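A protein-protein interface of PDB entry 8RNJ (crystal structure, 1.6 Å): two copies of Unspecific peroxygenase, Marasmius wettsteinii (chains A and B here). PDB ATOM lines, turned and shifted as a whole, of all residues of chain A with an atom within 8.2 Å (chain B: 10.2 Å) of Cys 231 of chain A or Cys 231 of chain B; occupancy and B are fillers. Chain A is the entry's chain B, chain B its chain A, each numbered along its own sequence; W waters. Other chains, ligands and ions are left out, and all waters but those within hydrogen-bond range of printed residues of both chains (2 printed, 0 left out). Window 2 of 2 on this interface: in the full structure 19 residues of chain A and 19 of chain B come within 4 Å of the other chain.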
ATOM      1  N   THR A 149     -38.157 -25.634  21.884  1.00  0.00           N
ATOM      2  CA  THR A 149     -36.771 -25.204  22.011  1.00  0.00           C
ATOM      3  C   THR A 149     -36.616 -24.577  23.391  1.00  0.00           C
ATOM      4  O   THR A 149     -37.355 -23.644  23.709  1.00  0.00           O
ATOM      5  CB  THR A 149     -36.357 -24.239  20.885  1.00  0.00           C
ATOM      6  OG1 THR A 149     -36.478 -24.906  19.627  1.00  0.00           O
ATOM      7  CG2 THR A 149     -34.930 -23.743  21.017  1.00  0.00           C
ATOM      8  N   ASN A 150     -35.648 -25.075  24.168  1.00  0.00           N
ATOM      9  CA  ASN A 150     -35.372 -24.598  25.513  1.00  0.00           C
ATOM     10  C   ASN A 150     -33.864 -24.573  25.737  1.00  0.00           C
ATOM     11  O   ASN A 150     -33.255 -25.634  25.894  1.00  0.00           O
ATOM     12  CB  ASN A 150     -36.047 -25.487  26.568  1.00  0.00           C
ATOM     13  CG  ASN A 150     -35.646 -25.122  27.976  1.00  0.00           C
ATOM     14  OD1 ASN A 150     -35.769 -23.966  28.380  1.00  0.00           O
ATOM     15  ND2 ASN A 150     -35.167 -26.097  28.739  1.00  0.00           N
ATOM     16  N   THR A 151     -33.280 -23.368  25.733  1.00  0.00           N
ATOM     17  CA  THR A 151     -31.842 -23.178  25.869  1.00  0.00           C
ATOM     18  C   THR A 151     -31.545 -22.167  26.968  1.00  0.00           C
ATOM     19  O   THR A 151     -32.455 -21.480  27.432  1.00  0.00           O
ATOM     20  CB  THR A 151     -31.237 -22.698  24.544  1.00  0.00           C
ATOM     21  OG1 THR A 151     -31.695 -21.374  24.278  1.00  0.00           O
ATOM     22  CG2 THR A 151     -31.603 -23.562  23.358  1.00  0.00           C
ATOM     23  N   ASP A 152     -30.263 -22.064  27.359  1.00  0.00           N
ATOM     24  CA  ASP A 152     -29.830 -21.019  28.276  1.00  0.00           C
ATOM     25  C   ASP A 152     -30.323 -19.660  27.767  1.00  0.00           C
ATOM     26  O   ASP A 152     -30.733 -18.820  28.558  1.00  0.00           O
ATOM     27  CB  ASP A 152     -28.304 -20.941  28.407  1.00  0.00           C
ATOM     28  CG  ASP A 152     -27.627 -22.137  29.045  1.00  0.00           C
ATOM     29  OD1 ASP A 152     -28.188 -22.667  30.026  1.00  0.00           O
ATOM     30  OD2 ASP A 152     -26.505 -22.487  28.590  1.00  0.00           O
ATOM     31  N   LEU A 153     -30.217 -19.423  26.458  1.00  0.00           N
ATOM     32  CA  LEU A 153     -30.606 -18.142  25.880  1.00  0.00           C
ATOM     33  C   LEU A 153     -32.116 -17.927  26.027  1.00  0.00           C
ATOM     34  O   LEU A 153     -32.534 -16.863  26.486  1.00  0.00           O
ATOM     35  CB  LEU A 153     -30.178 -18.042  24.411  1.00  0.00           C
ATOM     36  CG  LEU A 153     -30.619 -16.765  23.690  1.00  0.00           C
ATOM     37  CD1 LEU A 153     -30.006 -15.533  24.335  1.00  0.00           C
ATOM     38  CD2 LEU A 153     -30.275 -16.808  22.212  1.00  0.00           C
ATOM     39  N   THR A 154     -32.945 -18.899  25.622  1.00  0.00           N
ATOM     40  CA  THR A 154     -34.395 -18.701  25.724  1.00  0.00           C
ATOM     41  C   THR A 154     -34.810 -18.534  27.181  1.00  0.00           C
ATOM     42  O   THR A 154     -35.694 -17.729  27.475  1.00  0.00           O
ATOM     43  CB  THR A 154     -35.228 -19.795  25.035  1.00  0.00           C
ATOM     44  OG1 THR A 154     -35.035 -21.068  25.658  1.00  0.00           O
ATOM     45  CG2 THR A 154     -34.911 -19.923  23.561  1.00  0.00           C
ATOM     46  N   GLY A 228     -31.492 -30.344  26.617  1.00  0.00           N
ATOM     47  CA  GLY A 228     -31.027 -30.853  25.336  1.00  0.00           C
ATOM     48  C   GLY A 228     -29.828 -30.079  24.817  1.00  0.00           C
ATOM     49  O   GLY A 228     -29.046 -29.570  25.623  1.00  0.00           O
ATOM     50  N   ASP A 229     -29.660 -30.031  23.487  1.00  0.00           N
ATOM     51  CA  ASP A 229     -28.492 -29.382  22.889  1.00  0.00           C
ATOM     52  C   ASP A 229     -28.177 -28.078  23.617  1.00  0.00           C
ATOM     53  O   ASP A 229     -27.003 -27.756  23.833  1.00  0.00           O
ATOM     54  CB  ASP A 229     -28.662 -29.069  21.397  1.00  0.00           C
ATOM     55  CG  ASP A 229     -28.640 -30.276  20.474  1.00  0.00           C
ATOM     56  OD1 ASP A 229     -28.343 -31.402  20.956  1.00  0.00           O
ATOM     57  OD2 ASP A 229     -28.917 -30.070  19.261  1.00  0.00           O
ATOM     58  N   ASN A 230     -29.218 -27.327  23.985  1.00  0.00           N
ATOM     59  CA  ASN A 230     -28.951 -26.144  24.765  1.00  0.00           C
ATOM     60  C   ASN A 230     -28.055 -25.274  23.880  1.00  0.00           C
ATOM     61  O   ASN A 230     -27.162 -24.575  24.372  1.00  0.00           O
ATOM     62  CB  ASN A 230     -28.313 -26.547  26.102  1.00  0.00           C
ATOM     63  CG  ASN A 230     -28.183 -25.398  27.071  1.00  0.00           C
ATOM     64  OD1 ASN A 230     -28.295 -24.240  26.676  1.00  0.00           O
ATOM     65  ND2 ASN A 230     -27.935 -25.702  28.334  1.00  0.00           N
ATOM     66  N   CYS A 231     -28.252 -25.354  22.543  1.00  0.00           N
ATOM     67  CA  CYS A 231     -27.418 -24.525  21.664  1.00  0.00           C
ATOM     68  C   CYS A 231     -28.135 -23.197  21.444  1.00  0.00           C
ATOM     69  O   CYS A 231     -29.234 -23.155  20.896  1.00  0.00           O
ATOM     70  CB  CYS A 231     -27.010 -25.086  20.293  1.00  0.00           C
ATOM     71  SG  CYS A 231     -25.939 -23.989  19.247  1.00  0.00           S
ATOM     72  N   GLY A 232     -27.475 -22.118  21.877  1.00  0.00           N
ATOM     73  CA  GLY A 232     -28.106 -20.810  21.962  1.00  0.00           C
ATOM     74  C   GLY A 232     -27.952 -19.987  20.685  1.00  0.00           C
ATOM     75  O   GLY A 232     -27.709 -18.784  20.765  1.00  0.00           O
ATOM     76  N   ALA A 233     -28.092 -20.646  19.527  1.00  0.00           N
ATOM     77  CA  ALA A 233     -27.954 -20.020  18.220  1.00  0.00           C
ATOM     78  C   ALA A 233     -29.241 -19.279  17.871  1.00  0.00           C
ATOM     79  O   ALA A 233     -30.326 -19.841  18.013  1.00  0.00           O
ATOM     80  CB  ALA A 233     -27.648 -21.046  17.165  1.00  0.00           C
ATOM     81  N   ILE A 234     -29.111 -18.021  17.422  1.00  0.00           N
ATOM     82  CA  ILE A 234     -30.255 -17.266  16.941  1.00  0.00           C
ATOM     83  C   ILE A 234     -30.321 -17.355  15.418  1.00  0.00           C
ATOM     84  O   ILE A 234     -29.314 -17.555  14.730  1.00  0.00           O
ATOM     85  CB  ILE A 234     -30.242 -15.800  17.417  1.00  0.00           C
ATOM     86  CG1 ILE A 234     -29.021 -15.020  16.916  1.00  0.00           C
ATOM     87  CG2 ILE A 234     -30.360 -15.707  18.929  1.00  0.00           C
ATOM     88  CD1 ILE A 234     -29.251 -13.523  16.855  1.00  0.00           C
ATOM     89  N   GLY B  86     -16.493 -13.984  17.990  1.00  0.00           N
ATOM     90  CA  GLY B  86     -17.661 -14.849  18.060  1.00  0.00           C
ATOM     91  C   GLY B  86     -18.972 -14.164  17.666  1.00  0.00           C
ATOM     92  O   GLY B  86     -20.024 -14.782  17.768  1.00  0.00           O
ATOM     93  N   THR B  87     -18.920 -12.896  17.231  1.00  0.00           N
ATOM     94  CA  THR B  87     -20.051 -12.303  16.532  1.00  0.00           C
ATOM     95  C   THR B  87     -19.865 -12.613  15.046  1.00  0.00           C
ATOM     96  O   THR B  87     -20.422 -13.590  14.563  1.00  0.00           O
ATOM     97  CB  THR B  87     -20.264 -10.816  16.853  1.00  0.00           C
ATOM     98  OG1 THR B  87     -20.374 -10.643  18.270  1.00  0.00           O
ATOM     99  CG2 THR B  87     -21.493 -10.255  16.175  1.00  0.00           C
ATOM    100  N   VAL B 148      -9.827 -23.385  19.411  1.00  0.00           N
ATOM    101  CA  VAL B 148     -10.332 -23.094  18.069  1.00  0.00           C
ATOM    102  C   VAL B 148     -11.845 -23.317  18.024  1.00  0.00           C
ATOM    103  O   VAL B 148     -12.346 -24.305  18.566  1.00  0.00           O
ATOM    104  CB  VAL B 148      -9.590 -23.904  16.983  1.00  0.00           C
ATOM    105  CG1 VAL B 148      -9.676 -25.409  17.211  1.00  0.00           C
ATOM    106  CG2 VAL B 148     -10.072 -23.545  15.579  1.00  0.00           C
ATOM    107  N   THR B 149     -12.572 -22.378  17.387  1.00  0.00           N
ATOM    108  CA  THR B 149     -13.990 -22.525  17.094  1.00  0.00           C
ATOM    109  C   THR B 149     -14.142 -22.599  15.578  1.00  0.00           C
ATOM    110  O   THR B 149     -13.696 -21.712  14.861  1.00  0.00           O
ATOM    111  CB  THR B 149     -14.828 -21.386  17.689  1.00  0.00           C
ATOM    112  OG1 THR B 149     -14.621 -21.375  19.105  1.00  0.00           O
ATOM    113  CG2 THR B 149     -16.312 -21.529  17.410  1.00  0.00           C
ATOM    114  N   ASN B 150     -14.768 -23.676  15.109  1.00  0.00           N
ATOM    115  CA  ASN B 150     -14.873 -24.017  13.704  1.00  0.00           C
ATOM    116  C   ASN B 150     -16.206 -24.732  13.484  1.00  0.00           C
ATOM    117  O   ASN B 150     -16.348 -25.903  13.817  1.00  0.00           O
ATOM    118  CB  ASN B 150     -13.682 -24.865  13.259  1.00  0.00           C
ATOM    119  CG  ASN B 150     -13.899 -25.521  11.916  1.00  0.00           C
ATOM    120  OD1 ASN B 150     -14.258 -24.867  10.939  1.00  0.00           O
ATOM    121  ND2 ASN B 150     -13.681 -26.824  11.863  1.00  0.00           N
ATOM    122  N   THR B 151     -17.178 -23.995  12.937  1.00  0.00           N
ATOM    123  CA  THR B 151     -18.567 -24.420  12.848  1.00  0.00           C
ATOM    124  C   THR B 151     -19.083 -24.172  11.436  1.00  0.00           C
ATOM    125  O   THR B 151     -18.441 -23.470  10.653  1.00  0.00           O
ATOM    126  CB  THR B 151     -19.430 -23.639  13.849  1.00  0.00           C
ATOM    127  OG1 THR B 151     -19.499 -22.264  13.445  1.00  0.00           O
ATOM    128  CG2 THR B 151     -18.902 -23.718  15.265  1.00  0.00           C
ATOM    129  N   ASP B 152     -20.284 -24.689  11.138  1.00  0.00           N
ATOM    130  CA  ASP B 152     -20.957 -24.379   9.885  1.00  0.00           C
ATOM    131  C   ASP B 152     -20.982 -22.863   9.663  1.00  0.00           C
ATOM    132  O   ASP B 152     -20.750 -22.401   8.542  1.00  0.00           O
ATOM    133  CB  ASP B 152     -22.399 -24.889   9.832  1.00  0.00           C
ATOM    134  CG  ASP B 152     -22.584 -26.395   9.930  1.00  0.00           C
ATOM    135  OD1 ASP B 152     -21.764 -27.132   9.394  1.00  0.00           O
ATOM    136  OD2 ASP B 152     -23.606 -26.809  10.498  1.00  0.00           O
ATOM    137  N   LEU B 153     -21.270 -22.104  10.724  1.00  0.00           N
ATOM    138  CA  LEU B 153     -21.390 -20.657  10.600  1.00  0.00           C
ATOM    139  C   LEU B 153     -20.030 -20.036  10.268  1.00  0.00           C
ATOM    140  O   LEU B 153     -19.933 -19.258   9.316  1.00  0.00           O
ATOM    141  CB  LEU B 153     -21.967 -20.052  11.886  1.00  0.00           C
ATOM    142  CG  LEU B 153     -22.051 -18.523  11.902  1.00  0.00           C
ATOM    143  CD1 LEU B 153     -22.951 -18.011  10.799  1.00  0.00           C
ATOM    144  CD2 LEU B 153     -22.521 -18.027  13.266  1.00  0.00           C
ATOM    145  N   THR B 154     -18.985 -20.348  11.059  1.00  0.00           N
ATOM    146  CA  THR B 154     -17.679 -19.738  10.803  1.00  0.00           C
ATOM    147  C   THR B 154     -17.155 -20.143   9.424  1.00  0.00           C
ATOM    148  O   THR B 154     -16.520 -19.341   8.742  1.00  0.00           O
ATOM    149  CB  THR B 154     -16.641 -20.028  11.901  1.00  0.00           C
ATOM    150  OG1 THR B 154     -16.326 -21.421  11.905  1.00  0.00           O
ATOM    151  CG2 THR B 154     -17.106 -19.570  13.266  1.00  0.00           C
ATOM    152  N   ALA B 155     -17.405 -21.386   8.993  1.00  0.00           N
ATOM    153  CA  ALA B 155     -16.942 -21.849   7.686  1.00  0.00           C
ATOM    154  C   ALA B 155     -17.617 -21.075   6.559  1.00  0.00           C
ATOM    155  O   ALA B 155     -16.973 -20.763   5.554  1.00  0.00           O
ATOM    156  CB  ALA B 155     -17.193 -23.330   7.536  1.00  0.00           C
ATOM    157  N   ILE B 157     -18.925 -17.974   6.837  1.00  0.00           N
ATOM    158  CA  ILE B 157     -18.394 -16.620   6.894  1.00  0.00           C
ATOM    159  C   ILE B 157     -17.032 -16.587   6.200  1.00  0.00           C
ATOM    160  O   ILE B 157     -16.766 -15.687   5.418  1.00  0.00           O
ATOM    161  CB  ILE B 157     -18.324 -16.087   8.342  1.00  0.00           C
ATOM    162  CG1 ILE B 157     -19.726 -15.937   8.937  1.00  0.00           C
ATOM    163  CG2 ILE B 157     -17.547 -14.782   8.408  1.00  0.00           C
ATOM    164  CD1 ILE B 157     -19.754 -15.607  10.404  1.00  0.00           C
ATOM    165  N   TRP B 224     -13.547 -29.568   4.123  1.00  0.00           N
ATOM    166  CA  TRP B 224     -13.915 -29.028   5.424  1.00  0.00           C
ATOM    167  C   TRP B 224     -14.686 -30.052   6.268  1.00  0.00           C
ATOM    168  O   TRP B 224     -15.512 -30.788   5.737  1.00  0.00           O
ATOM    169  CB  TRP B 224     -14.746 -27.749   5.240  1.00  0.00           C
ATOM    170  CG  TRP B 224     -15.141 -27.125   6.541  1.00  0.00           C
ATOM    171  CD1 TRP B 224     -14.362 -26.357   7.355  1.00  0.00           C
ATOM    172  CD2 TRP B 224     -16.386 -27.304   7.235  1.00  0.00           C
ATOM    173  NE1 TRP B 224     -15.042 -26.042   8.499  1.00  0.00           N
ATOM    174  CE2 TRP B 224     -16.290 -26.598   8.448  1.00  0.00           C
ATOM    175  CE3 TRP B 224     -17.569 -28.000   6.960  1.00  0.00           C
ATOM    176  CZ2 TRP B 224     -17.326 -26.560   9.374  1.00  0.00           C
ATOM    177  CZ3 TRP B 224     -18.608 -27.933   7.861  1.00  0.00           C
ATOM    178  CH2 TRP B 224     -18.490 -27.221   9.051  1.00  0.00           C
ATOM    179  N   PRO B 226     -16.494 -29.811  10.564  1.00  0.00           N
ATOM    180  CA  PRO B 226     -16.604 -29.014  11.784  1.00  0.00           C
ATOM    181  C   PRO B 226     -15.751 -29.546  12.929  1.00  0.00           C
ATOM    182  O   PRO B 226     -15.326 -30.700  12.899  1.00  0.00           O
ATOM    183  CB  PRO B 226     -18.091 -29.138  12.152  1.00  0.00           C
ATOM    184  CG  PRO B 226     -18.499 -30.469  11.566  1.00  0.00           C
ATOM    185  CD  PRO B 226     -17.710 -30.590  10.280  1.00  0.00           C
ATOM    186  N   THR B 227     -15.592 -28.708  13.958  1.00  0.00           N
ATOM    187  CA  THR B 227     -14.917 -29.038  15.203  1.00  0.00           C
ATOM    188  C   THR B 227     -15.915 -29.046  16.367  1.00  0.00           C
ATOM    189  O   THR B 227     -16.731 -28.137  16.485  1.00  0.00           O
ATOM    190  CB  THR B 227     -13.816 -28.009  15.484  1.00  0.00           C
ATOM    191  OG1 THR B 227     -12.878 -28.084  14.415  1.00  0.00           O
ATOM    192  CG2 THR B 227     -13.128 -28.207  16.820  1.00  0.00           C
ATOM    193  N   GLY B 228     -15.832 -30.067  17.239  1.00  0.00           N
ATOM    194  CA  GLY B 228     -16.518 -30.048  18.521  1.00  0.00           C
ATOM    195  C   GLY B 228     -18.041 -30.071  18.381  1.00  0.00           C
ATOM    196  O   GLY B 228     -18.570 -30.837  17.590  1.00  0.00           O
ATOM    197  N   ASP B 229     -18.706 -29.181  19.127  1.00  0.00           N
ATOM    198  CA  ASP B 229     -20.152 -29.079  19.220  1.00  0.00           C
ATOM    199  C   ASP B 229     -20.777 -28.605  17.906  1.00  0.00           C
ATOM    200  O   ASP B 229     -21.968 -28.797  17.695  1.00  0.00           O
ATOM    201  CB  ASP B 229     -20.548 -28.105  20.342  1.00  0.00           C
ATOM    202  CG  ASP B 229     -20.233 -28.573  21.760  1.00  0.00           C
ATOM    203  OD1 ASP B 229     -19.976 -29.792  21.939  1.00  0.00           O
ATOM    204  OD2 ASP B 229     -20.225 -27.711  22.679  1.00  0.00           O
ATOM    205  N   ASN B 230     -19.997 -27.947  17.038  1.00  0.00           N
ATOM    206  CA  ASN B 230     -20.531 -27.352  15.819  1.00  0.00           C
ATOM    207  C   ASN B 230     -21.716 -26.436  16.158  1.00  0.00           C
ATOM    208  O   ASN B 230     -22.774 -26.516  15.544  1.00  0.00           O
ATOM    209  CB  ASN B 230     -20.898 -28.408  14.775  1.00  0.00           C
ATOM    210  CG  ASN B 230     -21.148 -27.828  13.398  1.00  0.00           C
ATOM    211  OD1 ASN B 230     -20.815 -26.666  13.133  1.00  0.00           O
ATOM    212  ND2 ASN B 230     -21.712 -28.634  12.517  1.00  0.00           N
ATOM    213  N   CYS B 231     -21.537 -25.570  17.152  1.00  0.00           N
ATOM    214  CA  CYS B 231     -22.603 -24.687  17.609  1.00  0.00           C
ATOM    215  C   CYS B 231     -22.517 -23.344  16.887  1.00  0.00           C
ATOM    216  O   CYS B 231     -21.531 -22.633  17.018  1.00  0.00           O
ATOM    217  CB  CYS B 231     -22.552 -24.477  19.119  1.00  0.00           C
ATOM    218  SG  CYS B 231     -23.867 -23.424  19.809  1.00  0.00           S
ATOM    219  N   GLY B 232     -23.600 -22.975  16.203  1.00  0.00           N
ATOM    220  CA  GLY B 232     -23.642 -21.759  15.403  1.00  0.00           C
ATOM    221  C   GLY B 232     -24.156 -20.541  16.169  1.00  0.00           C
ATOM    222  O   GLY B 232     -24.776 -19.677  15.553  1.00  0.00           O
ATOM    223  N   ALA B 233     -23.911 -20.485  17.489  1.00  0.00           N
ATOM    224  CA  ALA B 233     -24.361 -19.381  18.334  1.00  0.00           C
ATOM    225  C   ALA B 233     -23.411 -18.198  18.194  1.00  0.00           C
ATOM    226  O   ALA B 233     -22.201 -18.384  18.251  1.00  0.00           O
ATOM    227  CB  ALA B 233     -24.411 -19.826  19.779  1.00  0.00           C
ATOM    228  N   ILE B 234     -23.952 -16.988  17.997  1.00  0.00           N
ATOM    229  CA  ILE B 234     -23.141 -15.773  17.958  1.00  0.00           C
ATOM    230  C   ILE B 234     -23.220 -15.071  19.311  1.00  0.00           C
ATOM    231  O   ILE B 234     -24.198 -15.216  20.057  1.00  0.00           O
ATOM    232  CB  ILE B 234     -23.546 -14.820  16.811  1.00  0.00           C
ATOM    233  CG1 ILE B 234     -24.990 -14.320  16.921  1.00  0.00           C
ATOM    234  CG2 ILE B 234     -23.288 -15.455  15.454  1.00  0.00           C
ATOM    235  CD1 ILE B 234     -25.223 -12.999  16.216  1.00  0.00           C
ATOM    236  N   VAL B 235     -22.193 -14.268  19.593  1.00  0.00           N
ATOM    237  CA  VAL B 235     -22.159 -13.334  20.706  1.00  0.00           C
ATOM    238  C   VAL B 235     -23.056 -12.150  20.349  1.00  0.00           C
ATOM    239  O   VAL B 235     -22.927 -11.597  19.262  1.00  0.00           O
ATOM    240  CB  VAL B 235     -20.701 -12.910  20.988  1.00  0.00           C
ATOM    241  CG1 VAL B 235     -20.597 -11.751  21.966  1.00  0.00           C
ATOM    242  CG2 VAL B 235     -19.869 -14.103  21.448  1.00  0.00           C
ATOM    243  N   LEU B 236     -23.995 -11.794  21.237  1.00  0.00           N
ATOM    244  CA  LEU B 236     -25.074 -10.866  20.909  1.00  0.00           C
ATOM    245  C   LEU B 236     -24.771  -9.419  21.292  1.00  0.00           C
ATOM    246  O   LEU B 236     -25.517  -8.519  20.921  1.00  0.00           O
ATOM    247  CB  LEU B 236     -26.356 -11.340  21.595  1.00  0.00           C
ATOM    248  CG  LEU B 236     -26.897 -12.665  21.058  1.00  0.00           C
ATOM    249  CD1 LEU B 236     -28.088 -13.155  21.872  1.00  0.00           C
ATOM    250  CD2 LEU B 236     -27.278 -12.551  19.594  1.00  0.00           C
HETATM  251  O   HOH W   1     -26.790 -16.719  19.275  1.00  0.00           O
HETATM  252  O   HOH W   2     -26.609 -17.537  15.933  1.00  0.00           O
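SG of Cys 231 of chain B forms a disulfide with SG of Cys 231 of chain A.
N of Ala 233 of chain B sits close to SG of Cys 231 of chain B, at 3.7 Å.
The side-chain hydroxyl (OG1) of Thr 151 of chain A lies close to the backbone NH (N) of Leu 153 of chain A.
Leu 153 of chain A touches Leu 236 of chain B (CD1 to CD1, 3.9 Å).
Cys 231 of chain A touches Gly 232 of chain B.
Gly 232 of chain A touches Ala 233 of chain B (O to CB, 3.6 Å).
Ala 233 of chain A touches Gly 232 of chain B.
Ala 233 of chain A touches Ala 233 of chain B.
CD2 of Leu 236 of chain B touches CD1 of Ile 234 of chain A (3.5 Å).
Printed residues of chain B within 4 Å of Leu 153 of chain A: Leu 236.
Cys 231 of chain A touches just these residues of chain B: Cys 231 (2.2 Å) and Gly 232 (3.97 Å).
Of chain B, only Gly 232 and Ala 233 come within 4 Å of Ala 233 of chain A.
Printed residues of chain B within 4 Å of Ile 234 of chain A: Leu 236.
Thr 87 of chain B touches none of the printed residues of chain A.
Thr 227 of chain B touches none of the printed residues of chain A.
Of chain A, only Cys 231 (2.2 Å) comes within 4 Å of Cys 231 of chain B.
Printed residues of chain A within 4 Å of Gly 232 of chain B: Cys 231 (3.97 Å) and Ala 233 (3.6 Å).
Of the printed residues of chain A, Ala 233 of chain B touches Gly 232 and Ala 233.
Of the printed residues of chain A, Leu 236 of chain B touches Leu 153 and Ile 234.
The nearest printed residue of chain B that does not touch Leu 153 of chain A is Ile 234 of chain B (6.6 Å).
Printed residues of chain A that touch a printed residue of chain B: Leu 153, Cys 231, Gly 232, Ala 233 and Ile 234.
Hydrophobic or aromatic side chains of chain A that line the printed part of chain B: Leu 153, Ala 233 and Ile 234.
Printed residues of chain B that touch a printed residue of chain A: Cys 231, Gly 232, Ala 233 and Leu 236.
Hydrophobic or aromatic side chains of chain B that line the printed part of chain A: Ala 233 and Leu 236.
Among the printed residues, 7 pairs touch across the chains.
Cys 231 of chain B touches its own counterpart, Cys 231 of chain A.
Cys 231 of chain A touches Gly 232 of chain B, but with the chains exchanged Gly 232 of chain A does not touch Cys 231 of chain B (4.4 Å).
Gly 232 of chain A touches Ala 233 of chain B, and with the chains exchanged Ala 233 of chain A touches Gly 232 of chain B.
Ala 233 of chain B touches its own counterpart, Ala 233 of chain A.
Water W1 lies within hydrogen-bond range of O of Gly 232 of chain A, O of Ile 234 of chain B and N of Ile 234 of chain A.
Water W2 lies within hydrogen-bond range of O of Gly 232 of chain B, N of Ile 234 of chain A and N of Ile 234 of chain B.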
